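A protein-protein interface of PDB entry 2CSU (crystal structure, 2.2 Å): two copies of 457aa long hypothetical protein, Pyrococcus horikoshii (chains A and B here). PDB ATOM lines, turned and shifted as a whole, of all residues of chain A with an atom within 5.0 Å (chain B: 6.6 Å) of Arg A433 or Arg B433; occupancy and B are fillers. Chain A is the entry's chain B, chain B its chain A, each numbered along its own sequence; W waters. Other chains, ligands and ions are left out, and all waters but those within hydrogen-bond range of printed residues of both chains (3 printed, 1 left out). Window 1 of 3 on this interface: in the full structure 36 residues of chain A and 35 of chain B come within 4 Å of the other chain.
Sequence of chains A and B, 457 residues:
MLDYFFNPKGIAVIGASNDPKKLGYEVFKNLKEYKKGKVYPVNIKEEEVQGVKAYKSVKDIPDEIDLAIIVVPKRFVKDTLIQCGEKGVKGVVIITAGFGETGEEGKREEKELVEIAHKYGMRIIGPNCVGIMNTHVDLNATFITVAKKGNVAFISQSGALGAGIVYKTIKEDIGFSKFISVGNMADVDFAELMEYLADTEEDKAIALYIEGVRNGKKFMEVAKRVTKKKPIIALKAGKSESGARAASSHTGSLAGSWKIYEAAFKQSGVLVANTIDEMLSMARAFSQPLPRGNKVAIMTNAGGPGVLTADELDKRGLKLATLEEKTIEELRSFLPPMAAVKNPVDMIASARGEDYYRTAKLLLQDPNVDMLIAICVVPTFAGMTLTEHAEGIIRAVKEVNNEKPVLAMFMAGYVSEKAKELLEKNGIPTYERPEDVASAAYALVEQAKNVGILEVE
The side-chain carboxylate (OD2) of Asp B277 lies within salt-bridge range of the guanidinium group (NH1) of Arg A433 (2.9 Å). OD2 of Asp A277 is in salt-bridge range of NE of Arg B433, at 2.7 Å.
OD1 of Asp B277 is in salt-bridge range of NZ of Lys B168, at 2.9 Å. The side-chain hydroxyl (OG1) of Thr B275 sits close to the backbone NH (N) of Asp B277. The side-chain hydroxyl (OG1) of Thr B275 sits at hydrogen-bond distance from the backbone NH (N) of Glu B278 (3.0 Å). The guanidinium group of Arg B433 is in salt-bridge range of the side-chain carboxylate of Asp B277 (3.3 Å). The side-chain carboxylate (OD1) of Asp B436 lies within salt-bridge range of the guanidinium group (NH1) of Arg B433, at 3.0 Å. The guanidinium group (NH2) of Arg A433 is in salt-bridge range of the side-chain carboxylate (OD2) of Asp A436 (3.2 Å).
Among the printed residues, pairs that only touch across the chains: Glu A432 with Lys B168 (3.9 Å), Arg A433 with Arg B433 (3.5 Å) and Glu A435 with Thr B275 (3.4 Å).
Of chain B, only Asp B277 (2.8 Å) and Arg B433 (3.5 Å) come within 4 Å of Arg A433. Of chain A, only Asp A277 (2.7 Å) and Arg A433 (3.5 Å) come within 4 Å of Arg B433. Printed residues of chain A within 4 Å of Lys B168: Glu A432. Of the printed residues of chain B, Asp A277 touches Arg B433. Of the printed residues of chain A, Thr B275 touches Glu A435 (3.4 Å). Of the printed residues of chain B, Glu A432 touches Lys B168 (3.9 Å). Printed residues of chain A within 4 Å of Asp B277: Arg A433 (2.8 Å). Met A409 touches none of the printed residues of chain B. The nearest printed residue of chain B that does not touch Glu A432 is Glu B172 (5.3 Å).
Of the 10 printed residues of chain A, 4 touch a printed residue of chain B. Along chain B the printed residues that touch a printed residue of chain A span positions 168 to 433. Among the printed residues, Asp or Glu carboxylates within 4 Å of a Lys or Arg side-chain nitrogen of the other chain: Asp A277 with Arg B433 (2.7 Å) and Arg A433 with Asp B277 (2.9 Å).
Asp A277 touches Arg B433, and with the chains exchanged Arg A433 touches Asp B277. Arg A433 touches its own counterpart, Arg B433.
Water W2 lies within hydrogen-bond range of the side-chain carboxylate (OE2) of Glu B435 (2.7 Å) and the side-chain carboxylate (OD2) of Asp A277 (2.9 Å). Water W1 lies within hydrogen-bond range of OE2 of Glu A435 (2.7 Å), N of Asp B277 (3.1 Å) and N of Ile B276 (3.5 Å). Water W3 lies within hydrogen-bond range of OE1 of Glu A435 and N of Ile B276.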
ATOM      1  N   GLU A 172     -16.906 -19.748  -7.758  1.00  0.00           N
ATOM      2  CA  GLU A 172     -16.298 -20.579  -6.722  1.00  0.00           C
ATOM      3  C   GLU A 172     -14.787 -20.723  -6.905  1.00  0.00           C
ATOM      4  O   GLU A 172     -14.161 -21.624  -6.333  1.00  0.00           O
ATOM      5  CB  GLU A 172     -16.939 -21.970  -6.695  1.00  0.00           C
ATOM      6  CG  GLU A 172     -18.412 -21.993  -6.319  1.00  0.00           C
ATOM      7  CD  GLU A 172     -18.879 -23.377  -5.895  1.00  0.00           C
ATOM      8  OE1 GLU A 172     -18.573 -24.353  -6.610  1.00  0.00           O
ATOM      9  OE2 GLU A 172     -19.551 -23.491  -4.848  1.00  0.00           O
ATOM     10  N   ASP A 277     -21.883 -30.565  -6.343  1.00  0.00           N
ATOM     11  CA  ASP A 277     -20.723 -30.244  -5.522  1.00  0.00           C
ATOM     12  C   ASP A 277     -19.815 -31.454  -5.228  1.00  0.00           C
ATOM     13  O   ASP A 277     -18.614 -31.295  -5.043  1.00  0.00           O
ATOM     14  CB  ASP A 277     -21.168 -29.544  -4.228  1.00  0.00           C
ATOM     15  CG  ASP A 277     -21.405 -28.037  -4.429  1.00  0.00           C
ATOM     16  OD1 ASP A 277     -20.438 -27.320  -4.762  1.00  0.00           O
ATOM     17  OD2 ASP A 277     -22.550 -27.563  -4.261  1.00  0.00           O
ATOM     18  N   MET A 409      -9.619 -26.569   3.992  1.00  0.00           N
ATOM     19  CA  MET A 409     -10.982 -26.123   4.201  1.00  0.00           C
ATOM     20  C   MET A 409     -10.999 -24.862   5.055  1.00  0.00           C
ATOM     21  O   MET A 409     -10.996 -24.896   6.276  1.00  0.00           O
ATOM     22  CB  MET A 409     -11.761 -27.232   4.905  1.00  0.00           C
ATOM     23  CG  MET A 409     -13.232 -27.272   4.494  1.00  0.00           C
ATOM     24  SD  MET A 409     -14.345 -27.159   5.901  1.00  0.00           S
ATOM     25  CE  MET A 409     -14.721 -25.404   5.777  1.00  0.00           C
ATOM     26  N   TYR A 431     -11.676 -26.153   0.254  1.00  0.00           N
ATOM     27  CA  TYR A 431     -13.130 -26.176   0.258  1.00  0.00           C
ATOM     28  C   TYR A 431     -13.706 -25.335   1.395  1.00  0.00           C
ATOM     29  O   TYR A 431     -12.972 -24.856   2.264  1.00  0.00           O
ATOM     30  CB  TYR A 431     -13.632 -27.621   0.348  1.00  0.00           C
ATOM     31  CG  TYR A 431     -13.012 -28.525  -0.701  1.00  0.00           C
ATOM     32  CD1 TYR A 431     -11.720 -29.025  -0.535  1.00  0.00           C
ATOM     33  CD2 TYR A 431     -13.690 -28.821  -1.887  1.00  0.00           C
ATOM     34  CE1 TYR A 431     -11.112 -29.791  -1.519  1.00  0.00           C
ATOM     35  CE2 TYR A 431     -13.088 -29.594  -2.884  1.00  0.00           C
ATOM     36  CZ  TYR A 431     -11.796 -30.073  -2.691  1.00  0.00           C
ATOM     37  OH  TYR A 431     -11.178 -30.836  -3.662  1.00  0.00           O
ATOM     38  N   GLU A 432     -15.025 -25.165   1.377  1.00  0.00           N
ATOM     39  CA  GLU A 432     -15.726 -24.363   2.373  1.00  0.00           C
ATOM     40  C   GLU A 432     -16.739 -25.202   3.149  1.00  0.00           C
ATOM     41  O   GLU A 432     -17.365 -24.730   4.094  1.00  0.00           O
ATOM     42  CB  GLU A 432     -16.407 -23.174   1.659  1.00  0.00           C
ATOM     43  CG  GLU A 432     -17.248 -22.229   2.526  1.00  0.00           C
ATOM     44  CD  GLU A 432     -17.440 -20.841   1.876  1.00  0.00           C
ATOM     45  OE1 GLU A 432     -18.439 -20.153   2.186  1.00  0.00           O
ATOM     46  OE2 GLU A 432     -16.578 -20.437   1.060  1.00  0.00           O
ATOM     47  N   ARG A 433     -16.877 -26.465   2.768  1.00  0.00           N
ATOM     48  CA  ARG A 433     -17.830 -27.336   3.435  1.00  0.00           C
ATOM     49  C   ARG A 433     -17.202 -28.646   3.901  1.00  0.00           C
ATOM     50  O   ARG A 433     -16.422 -29.264   3.183  1.00  0.00           O
ATOM     51  CB  ARG A 433     -19.018 -27.640   2.501  1.00  0.00           C
ATOM     52  CG  ARG A 433     -19.712 -26.391   1.921  1.00  0.00           C
ATOM     53  CD  ARG A 433     -21.137 -26.690   1.439  1.00  0.00           C
ATOM     54  NE  ARG A 433     -21.181 -27.835   0.537  1.00  0.00           N
ATOM     55  CZ  ARG A 433     -22.299 -28.407   0.101  1.00  0.00           C
ATOM     56  NH1 ARG A 433     -23.484 -27.942   0.474  1.00  0.00           N
ATOM     57  NH2 ARG A 433     -22.229 -29.465  -0.695  1.00  0.00           N
ATOM     58  N   PRO A 434     -17.524 -29.070   5.132  1.00  0.00           N
ATOM     59  CA  PRO A 434     -16.988 -30.318   5.681  1.00  0.00           C
ATOM     60  C   PRO A 434     -17.211 -31.471   4.708  1.00  0.00           C
ATOM     61  O   PRO A 434     -16.264 -32.150   4.320  1.00  0.00           O
ATOM     62  CB  PRO A 434     -17.784 -30.489   6.971  1.00  0.00           C
ATOM     63  CG  PRO A 434     -17.935 -29.064   7.431  1.00  0.00           C
ATOM     64  CD  PRO A 434     -18.314 -28.347   6.148  1.00  0.00           C
ATOM     65  N   GLU A 435     -18.463 -31.670   4.302  1.00  0.00           N
ATOM     66  CA  GLU A 435     -18.808 -32.747   3.379  1.00  0.00           C
ATOM     67  C   GLU A 435     -17.999 -32.706   2.090  1.00  0.00           C
ATOM     68  O   GLU A 435     -17.762 -33.745   1.480  1.00  0.00           O
ATOM     69  CB  GLU A 435     -20.301 -32.711   3.035  1.00  0.00           C
ATOM     70  CG  GLU A 435     -20.776 -31.394   2.416  1.00  0.00           C
ATOM     71  CD  GLU A 435     -21.363 -30.446   3.443  1.00  0.00           C
ATOM     72  OE1 GLU A 435     -20.728 -30.248   4.509  1.00  0.00           O
ATOM     73  OE2 GLU A 435     -22.461 -29.897   3.183  1.00  0.00           O
ATOM     74  N   ASP A 436     -17.559 -31.517   1.684  1.00  0.00           N
ATOM     75  CA  ASP A 436     -16.793 -31.371   0.447  1.00  0.00           C
ATOM     76  C   ASP A 436     -15.340 -31.831   0.502  1.00  0.00           C
ATOM     77  O   ASP A 436     -14.898 -32.585  -0.366  1.00  0.00           O
ATOM     78  CB  ASP A 436     -16.847 -29.924  -0.033  1.00  0.00           C
ATOM     79  CG  ASP A 436     -18.226 -29.531  -0.572  1.00  0.00           C
ATOM     80  OD1 ASP A 436     -18.381 -28.362  -0.969  1.00  0.00           O
ATOM     81  OD2 ASP A 436     -19.146 -30.380  -0.601  1.00  0.00           O
ATOM     82  N   VAL A 437     -14.593 -31.381   1.508  1.00  0.00           N
ATOM     83  CA  VAL A 437     -13.201 -31.786   1.641  1.00  0.00           C
ATOM     84  C   VAL A 437     -13.149 -33.311   1.851  1.00  0.00           C
ATOM     85  O   VAL A 437     -12.247 -34.000   1.353  1.00  0.00           O
ATOM     86  CB  VAL A 437     -12.510 -31.023   2.818  1.00  0.00           C
ATOM     87  CG1 VAL A 437     -13.183 -31.348   4.147  1.00  0.00           C
ATOM     88  CG2 VAL A 437     -11.015 -31.347   2.855  1.00  0.00           C
ATOM     89  N   LYS B 168     -20.266 -17.231   5.999  1.00  0.00           N
ATOM     90  CA  LYS B 168     -20.842 -17.993   4.910  1.00  0.00           C
ATOM     91  C   LYS B 168     -22.112 -17.338   4.403  1.00  0.00           C
ATOM     92  O   LYS B 168     -22.221 -17.008   3.228  1.00  0.00           O
ATOM     93  CB  LYS B 168     -21.159 -19.418   5.365  1.00  0.00           C
ATOM     94  CG  LYS B 168     -21.715 -20.312   4.247  1.00  0.00           C
ATOM     95  CD  LYS B 168     -21.941 -21.739   4.740  1.00  0.00           C
ATOM     96  CE  LYS B 168     -21.983 -22.738   3.591  1.00  0.00           C
ATOM     97  NZ  LYS B 168     -23.137 -22.608   2.671  1.00  0.00           N
ATOM     98  N   GLU B 172     -23.497 -15.479   0.901  1.00  0.00           N
ATOM     99  CA  GLU B 172     -24.614 -16.164   0.245  1.00  0.00           C
ATOM    100  C   GLU B 172     -25.889 -15.349   0.355  1.00  0.00           C
ATOM    101  O   GLU B 172     -26.960 -15.784  -0.069  1.00  0.00           O
ATOM    102  CB  GLU B 172     -24.843 -17.551   0.864  1.00  0.00           C
ATOM    103  CG  GLU B 172     -23.741 -18.565   0.578  1.00  0.00           C
ATOM    104  CD  GLU B 172     -24.041 -19.934   1.170  1.00  0.00           C
ATOM    105  OE1 GLU B 172     -24.823 -19.997   2.136  1.00  0.00           O
ATOM    106  OE2 GLU B 172     -23.488 -20.939   0.680  1.00  0.00           O
ATOM    107  N   THR B 275     -26.060 -31.380   7.634  1.00  0.00           N
ATOM    108  CA  THR B 275     -24.989 -30.484   7.201  1.00  0.00           C
ATOM    109  C   THR B 275     -25.368 -29.035   7.502  1.00  0.00           C
ATOM    110  O   THR B 275     -26.530 -28.719   7.792  1.00  0.00           O
ATOM    111  CB  THR B 275     -24.685 -30.559   5.681  1.00  0.00           C
ATOM    112  OG1 THR B 275     -25.736 -29.918   4.954  1.00  0.00           O
ATOM    113  CG2 THR B 275     -24.529 -32.011   5.213  1.00  0.00           C
ATOM    114  N   ILE B 276     -24.374 -28.159   7.434  1.00  0.00           N
ATOM    115  CA  ILE B 276     -24.572 -26.744   7.662  1.00  0.00           C
ATOM    116  C   ILE B 276     -25.620 -26.263   6.667  1.00  0.00           C
ATOM    117  O   ILE B 276     -26.666 -25.732   7.056  1.00  0.00           O
ATOM    118  CB  ILE B 276     -23.231 -25.989   7.458  1.00  0.00           C
ATOM    119  CG1 ILE B 276     -22.277 -26.343   8.601  1.00  0.00           C
ATOM    120  CG2 ILE B 276     -23.452 -24.471   7.423  1.00  0.00           C
ATOM    121  CD1 ILE B 276     -20.797 -25.997   8.311  1.00  0.00           C
ATOM    122  N   ASP B 277     -25.353 -26.495   5.384  1.00  0.00           N
ATOM    123  CA  ASP B 277     -26.252 -26.080   4.323  1.00  0.00           C
ATOM    124  C   ASP B 277     -27.684 -26.558   4.477  1.00  0.00           C
ATOM    125  O   ASP B 277     -28.613 -25.813   4.174  1.00  0.00           O
ATOM    126  CB  ASP B 277     -25.683 -26.482   2.954  1.00  0.00           C
ATOM    127  CG  ASP B 277     -24.818 -25.378   2.350  1.00  0.00           C
ATOM    128  OD1 ASP B 277     -25.373 -24.300   2.074  1.00  0.00           O
ATOM    129  OD2 ASP B 277     -23.599 -25.568   2.161  1.00  0.00           O
ATOM    130  N   GLU B 278     -27.874 -27.781   4.964  1.00  0.00           N
ATOM    131  CA  GLU B 278     -29.223 -28.287   5.162  1.00  0.00           C
ATOM    132  C   GLU B 278     -29.897 -27.512   6.276  1.00  0.00           C
ATOM    133  O   GLU B 278     -31.060 -27.136   6.158  1.00  0.00           O
ATOM    134  CB  GLU B 278     -29.213 -29.777   5.531  1.00  0.00           C
ATOM    135  CG  GLU B 278     -28.694 -30.701   4.436  1.00  0.00           C
ATOM    136  CD  GLU B 278     -28.875 -32.178   4.791  1.00  0.00           C
ATOM    137  OE1 GLU B 278     -29.390 -32.480   5.898  1.00  0.00           O
ATOM    138  OE2 GLU B 278     -28.499 -33.035   3.962  1.00  0.00           O
ATOM    139  N   SER B 281     -30.682 -24.133   4.883  1.00  0.00           N
ATOM    140  CA  SER B 281     -31.665 -24.226   3.816  1.00  0.00           C
ATOM    141  C   SER B 281     -33.048 -24.531   4.373  1.00  0.00           C
ATOM    142  O   SER B 281     -34.054 -23.975   3.907  1.00  0.00           O
ATOM    143  CB  SER B 281     -31.262 -25.302   2.806  1.00  0.00           C
ATOM    144  OG  SER B 281     -29.938 -25.113   2.322  1.00  0.00           O
ATOM    145  N   THR B 309     -33.365 -31.992  -9.201  1.00  0.00           N
ATOM    146  CA  THR B 309     -34.243 -31.537  -8.130  1.00  0.00           C
ATOM    147  C   THR B 309     -35.337 -32.559  -7.838  1.00  0.00           C
ATOM    148  O   THR B 309     -35.719 -32.757  -6.682  1.00  0.00           O
ATOM    149  CB  THR B 309     -34.931 -30.203  -8.448  1.00  0.00           C
ATOM    150  OG1 THR B 309     -33.950 -29.183  -8.692  1.00  0.00           O
ATOM    151  CG2 THR B 309     -35.794 -29.799  -7.276  1.00  0.00           C
ATOM    152  N   GLU B 312     -33.806 -35.361  -5.668  1.00  0.00           N
ATOM    153  CA  GLU B 312     -33.616 -34.862  -4.312  1.00  0.00           C
ATOM    154  C   GLU B 312     -34.886 -34.790  -3.492  1.00  0.00           C
ATOM    155  O   GLU B 312     -34.869 -35.055  -2.289  1.00  0.00           O
ATOM    156  CB  GLU B 312     -32.959 -33.482  -4.343  1.00  0.00           C
ATOM    157  CG  GLU B 312     -31.502 -33.491  -4.783  1.00  0.00           C
ATOM    158  CD  GLU B 312     -30.614 -34.324  -3.862  1.00  0.00           C
ATOM    159  OE1 GLU B 312     -30.954 -34.489  -2.670  1.00  0.00           O
ATOM    160  OE2 GLU B 312     -29.563 -34.798  -4.335  1.00  0.00           O
ATOM    161  N   MET B 409     -34.950 -22.001  -7.168  1.00  0.00           N
ATOM    162  CA  MET B 409     -33.571 -22.420  -7.329  1.00  0.00           C
ATOM    163  C   MET B 409     -32.981 -21.837  -8.607  1.00  0.00           C
ATOM    164  O   MET B 409     -33.300 -22.249  -9.715  1.00  0.00           O
ATOM    165  CB  MET B 409     -33.541 -23.948  -7.392  1.00  0.00           C
ATOM    166  CG  MET B 409     -32.165 -24.521  -7.045  1.00  0.00           C
ATOM    167  SD  MET B 409     -31.434 -25.417  -8.421  1.00  0.00           S
ATOM    168  CE  MET B 409     -29.940 -24.431  -8.592  1.00  0.00           C
ATOM    169  N   PHE B 410     -32.136 -20.811  -8.414  1.00  0.00           N
ATOM    170  CA  PHE B 410     -31.611 -20.090  -9.568  1.00  0.00           C
ATOM    171  C   PHE B 410     -30.117 -20.343  -9.775  1.00  0.00           C
ATOM    172  O   PHE B 410     -29.330 -20.425  -8.840  1.00  0.00           O
ATOM    173  CB  PHE B 410     -31.860 -18.599  -9.345  1.00  0.00           C
ATOM    174  CG  PHE B 410     -33.176 -18.205  -9.945  1.00  0.00           C
ATOM    175  CD1 PHE B 410     -34.323 -18.915  -9.614  1.00  0.00           C
ATOM    176  CD2 PHE B 410     -33.243 -17.126 -10.811  1.00  0.00           C
ATOM    177  CE1 PHE B 410     -35.544 -18.537 -10.151  1.00  0.00           C
ATOM    178  CE2 PHE B 410     -34.474 -16.751 -11.345  1.00  0.00           C
ATOM    179  CZ  PHE B 410     -35.627 -17.453 -11.017  1.00  0.00           C
ATOM    180  N   MET B 411     -29.740 -20.500 -11.059  1.00  0.00           N
ATOM    181  CA  MET B 411     -28.335 -20.729 -11.376  1.00  0.00           C
ATOM    182  C   MET B 411     -27.860 -19.809 -12.503  1.00  0.00           C
ATOM    183  O   MET B 411     -28.515 -19.630 -13.520  1.00  0.00           O
ATOM    184  CB  MET B 411     -28.176 -22.189 -11.800  1.00  0.00           C
ATOM    185  CG  MET B 411     -28.363 -23.163 -10.635  1.00  0.00           C
ATOM    186  SD  MET B 411     -28.276 -24.880 -11.160  1.00  0.00           S
ATOM    187  CE  MET B 411     -26.566 -24.879 -11.723  1.00  0.00           C
ATOM    188  N   TYR B 431     -32.395 -20.853  -3.677  1.00  0.00           N
ATOM    189  CA  TYR B 431     -31.267 -21.752  -3.525  1.00  0.00           C
ATOM    190  C   TYR B 431     -30.474 -21.898  -4.799  1.00  0.00           C
ATOM    191  O   TYR B 431     -30.940 -21.531  -5.864  1.00  0.00           O
ATOM    192  CB  TYR B 431     -31.778 -23.112  -3.032  1.00  0.00           C
ATOM    193  CG  TYR B 431     -32.592 -22.976  -1.762  1.00  0.00           C
ATOM    194  CD1 TYR B 431     -33.935 -22.578  -1.802  1.00  0.00           C
ATOM    195  CD2 TYR B 431     -32.005 -23.186  -0.519  1.00  0.00           C
ATOM    196  CE1 TYR B 431     -34.668 -22.396  -0.624  1.00  0.00           C
ATOM    197  CE2 TYR B 431     -32.722 -23.002   0.656  1.00  0.00           C
ATOM    198  CZ  TYR B 431     -34.049 -22.611   0.603  1.00  0.00           C
ATOM    199  OH  TYR B 431     -34.747 -22.442   1.779  1.00  0.00           O
ATOM    200  N   GLU B 432     -29.273 -22.446  -4.680  1.00  0.00           N
ATOM    201  CA  GLU B 432     -28.400 -22.620  -5.829  1.00  0.00           C
ATOM    202  C   GLU B 432     -28.112 -24.101  -6.051  1.00  0.00           C
ATOM    203  O   GLU B 432     -27.427 -24.466  -7.006  1.00  0.00           O
ATOM    204  CB  GLU B 432     -27.090 -21.827  -5.604  1.00  0.00           C
ATOM    205  CG  GLU B 432     -26.030 -21.976  -6.696  1.00  0.00           C
ATOM    206  CD  GLU B 432     -25.102 -20.757  -6.814  1.00  0.00           C
ATOM    207  OE1 GLU B 432     -23.984 -20.899  -7.366  1.00  0.00           O
ATOM    208  OE2 GLU B 432     -25.498 -19.653  -6.370  1.00  0.00           O
ATOM    209  N   ARG B 433     -28.661 -24.942  -5.180  1.00  0.00           N
ATOM    210  CA  ARG B 433     -28.455 -26.390  -5.256  1.00  0.00           C
ATOM    211  C   ARG B 433     -29.748 -27.201  -5.252  1.00  0.00           C
ATOM    212  O   ARG B 433     -30.679 -26.895  -4.525  1.00  0.00           O
ATOM    213  CB  ARG B 433     -27.629 -26.885  -4.066  1.00  0.00           C
ATOM    214  CG  ARG B 433     -26.287 -26.209  -3.859  1.00  0.00           C
ATOM    215  CD  ARG B 433     -25.538 -26.906  -2.741  1.00  0.00           C
ATOM    216  NE  ARG B 433     -24.202 -26.364  -2.568  1.00  0.00           N
ATOM    217  CZ  ARG B 433     -23.909 -25.310  -1.813  1.00  0.00           C
ATOM    218  NH1 ARG B 433     -24.875 -24.684  -1.146  1.00  0.00           N
ATOM    219  NH2 ARG B 433     -22.650 -24.881  -1.729  1.00  0.00           N
ATOM    220  N   PRO B 434     -29.810 -28.259  -6.063  1.00  0.00           N
ATOM    221  CA  PRO B 434     -31.024 -29.074  -6.079  1.00  0.00           C
ATOM    222  C   PRO B 434     -31.285 -29.651  -4.687  1.00  0.00           C
ATOM    223  O   PRO B 434     -32.425 -29.685  -4.232  1.00  0.00           O
ATOM    224  CB  PRO B 434     -30.691 -30.153  -7.105  1.00  0.00           C
ATOM    225  CG  PRO B 434     -29.870 -29.402  -8.094  1.00  0.00           C
ATOM    226  CD  PRO B 434     -28.935 -28.606  -7.196  1.00  0.00           C
ATOM    227  N   GLU B 435     -30.225 -30.080  -4.000  1.00  0.00           N
ATOM    228  CA  GLU B 435     -30.398 -30.653  -2.663  1.00  0.00           C
ATOM    229  C   GLU B 435     -30.865 -29.632  -1.635  1.00  0.00           C
ATOM    230  O   GLU B 435     -31.613 -29.964  -0.715  1.00  0.00           O
ATOM    231  CB  GLU B 435     -29.101 -31.319  -2.177  1.00  0.00           C
ATOM    232  CG  GLU B 435     -27.861 -30.441  -2.223  1.00  0.00           C
ATOM    233  CD  GLU B 435     -27.202 -30.451  -3.578  1.00  0.00           C
ATOM    234  OE1 GLU B 435     -27.939 -30.498  -4.599  1.00  0.00           O
ATOM    235  OE2 GLU B 435     -25.947 -30.403  -3.624  1.00  0.00           O
ATOM    236  N   ASP B 436     -30.438 -28.388  -1.799  1.00  0.00           N
ATOM    237  CA  ASP B 436     -30.816 -27.324  -0.870  1.00  0.00           C
ATOM    238  C   ASP B 436     -32.298 -26.969  -0.958  1.00  0.00           C
ATOM    239  O   ASP B 436     -32.978 -26.852   0.063  1.00  0.00           O
ATOM    240  CB  ASP B 436     -29.965 -26.078  -1.139  1.00  0.00           C
ATOM    241  CG  ASP B 436     -28.536 -26.213  -0.609  1.00  0.00           C
ATOM    242  OD1 ASP B 436     -27.769 -25.229  -0.695  1.00  0.00           O
ATOM    243  OD2 ASP B 436     -28.181 -27.296  -0.106  1.00  0.00           O
ATOM    244  N   VAL B 437     -32.812 -26.795  -2.175  1.00  0.00           N
ATOM    245  CA  VAL B 437     -34.221 -26.458  -2.329  1.00  0.00           C
ATOM    246  C   VAL B 437     -35.061 -27.665  -1.867  1.00  0.00           C
ATOM    247  O   VAL B 437     -36.123 -27.495  -1.278  1.00  0.00           O
ATOM    248  CB  VAL B 437     -34.543 -26.039  -3.818  1.00  0.00           C
ATOM    249  CG1 VAL B 437     -34.276 -27.183  -4.777  1.00  0.00           C
ATOM    250  CG2 VAL B 437     -35.993 -25.539  -3.939  1.00  0.00           C
ATOM    251  N   ALA B 438     -34.567 -28.879  -2.102  1.00  0.00           N
ATOM    252  CA  ALA B 438     -35.285 -30.087  -1.671  1.00  0.00           C
ATOM    253  C   ALA B 438     -35.352 -30.134  -0.150  1.00  0.00           C
ATOM    254  O   ALA B 438     -36.377 -30.490   0.422  1.00  0.00           O
ATOM    255  CB  ALA B 438     -34.585 -31.371  -2.207  1.00  0.00           C
HETATM  256  O   HOH W   1     -22.599 -27.532   4.510  1.00  0.00           O
HETATM  257  O   HOH W   2     -24.550 -29.244  -5.586  1.00  0.00           O
HETATM  258  O   HOH W   3     -21.570 -29.412   7.277  1.00  0.00           O
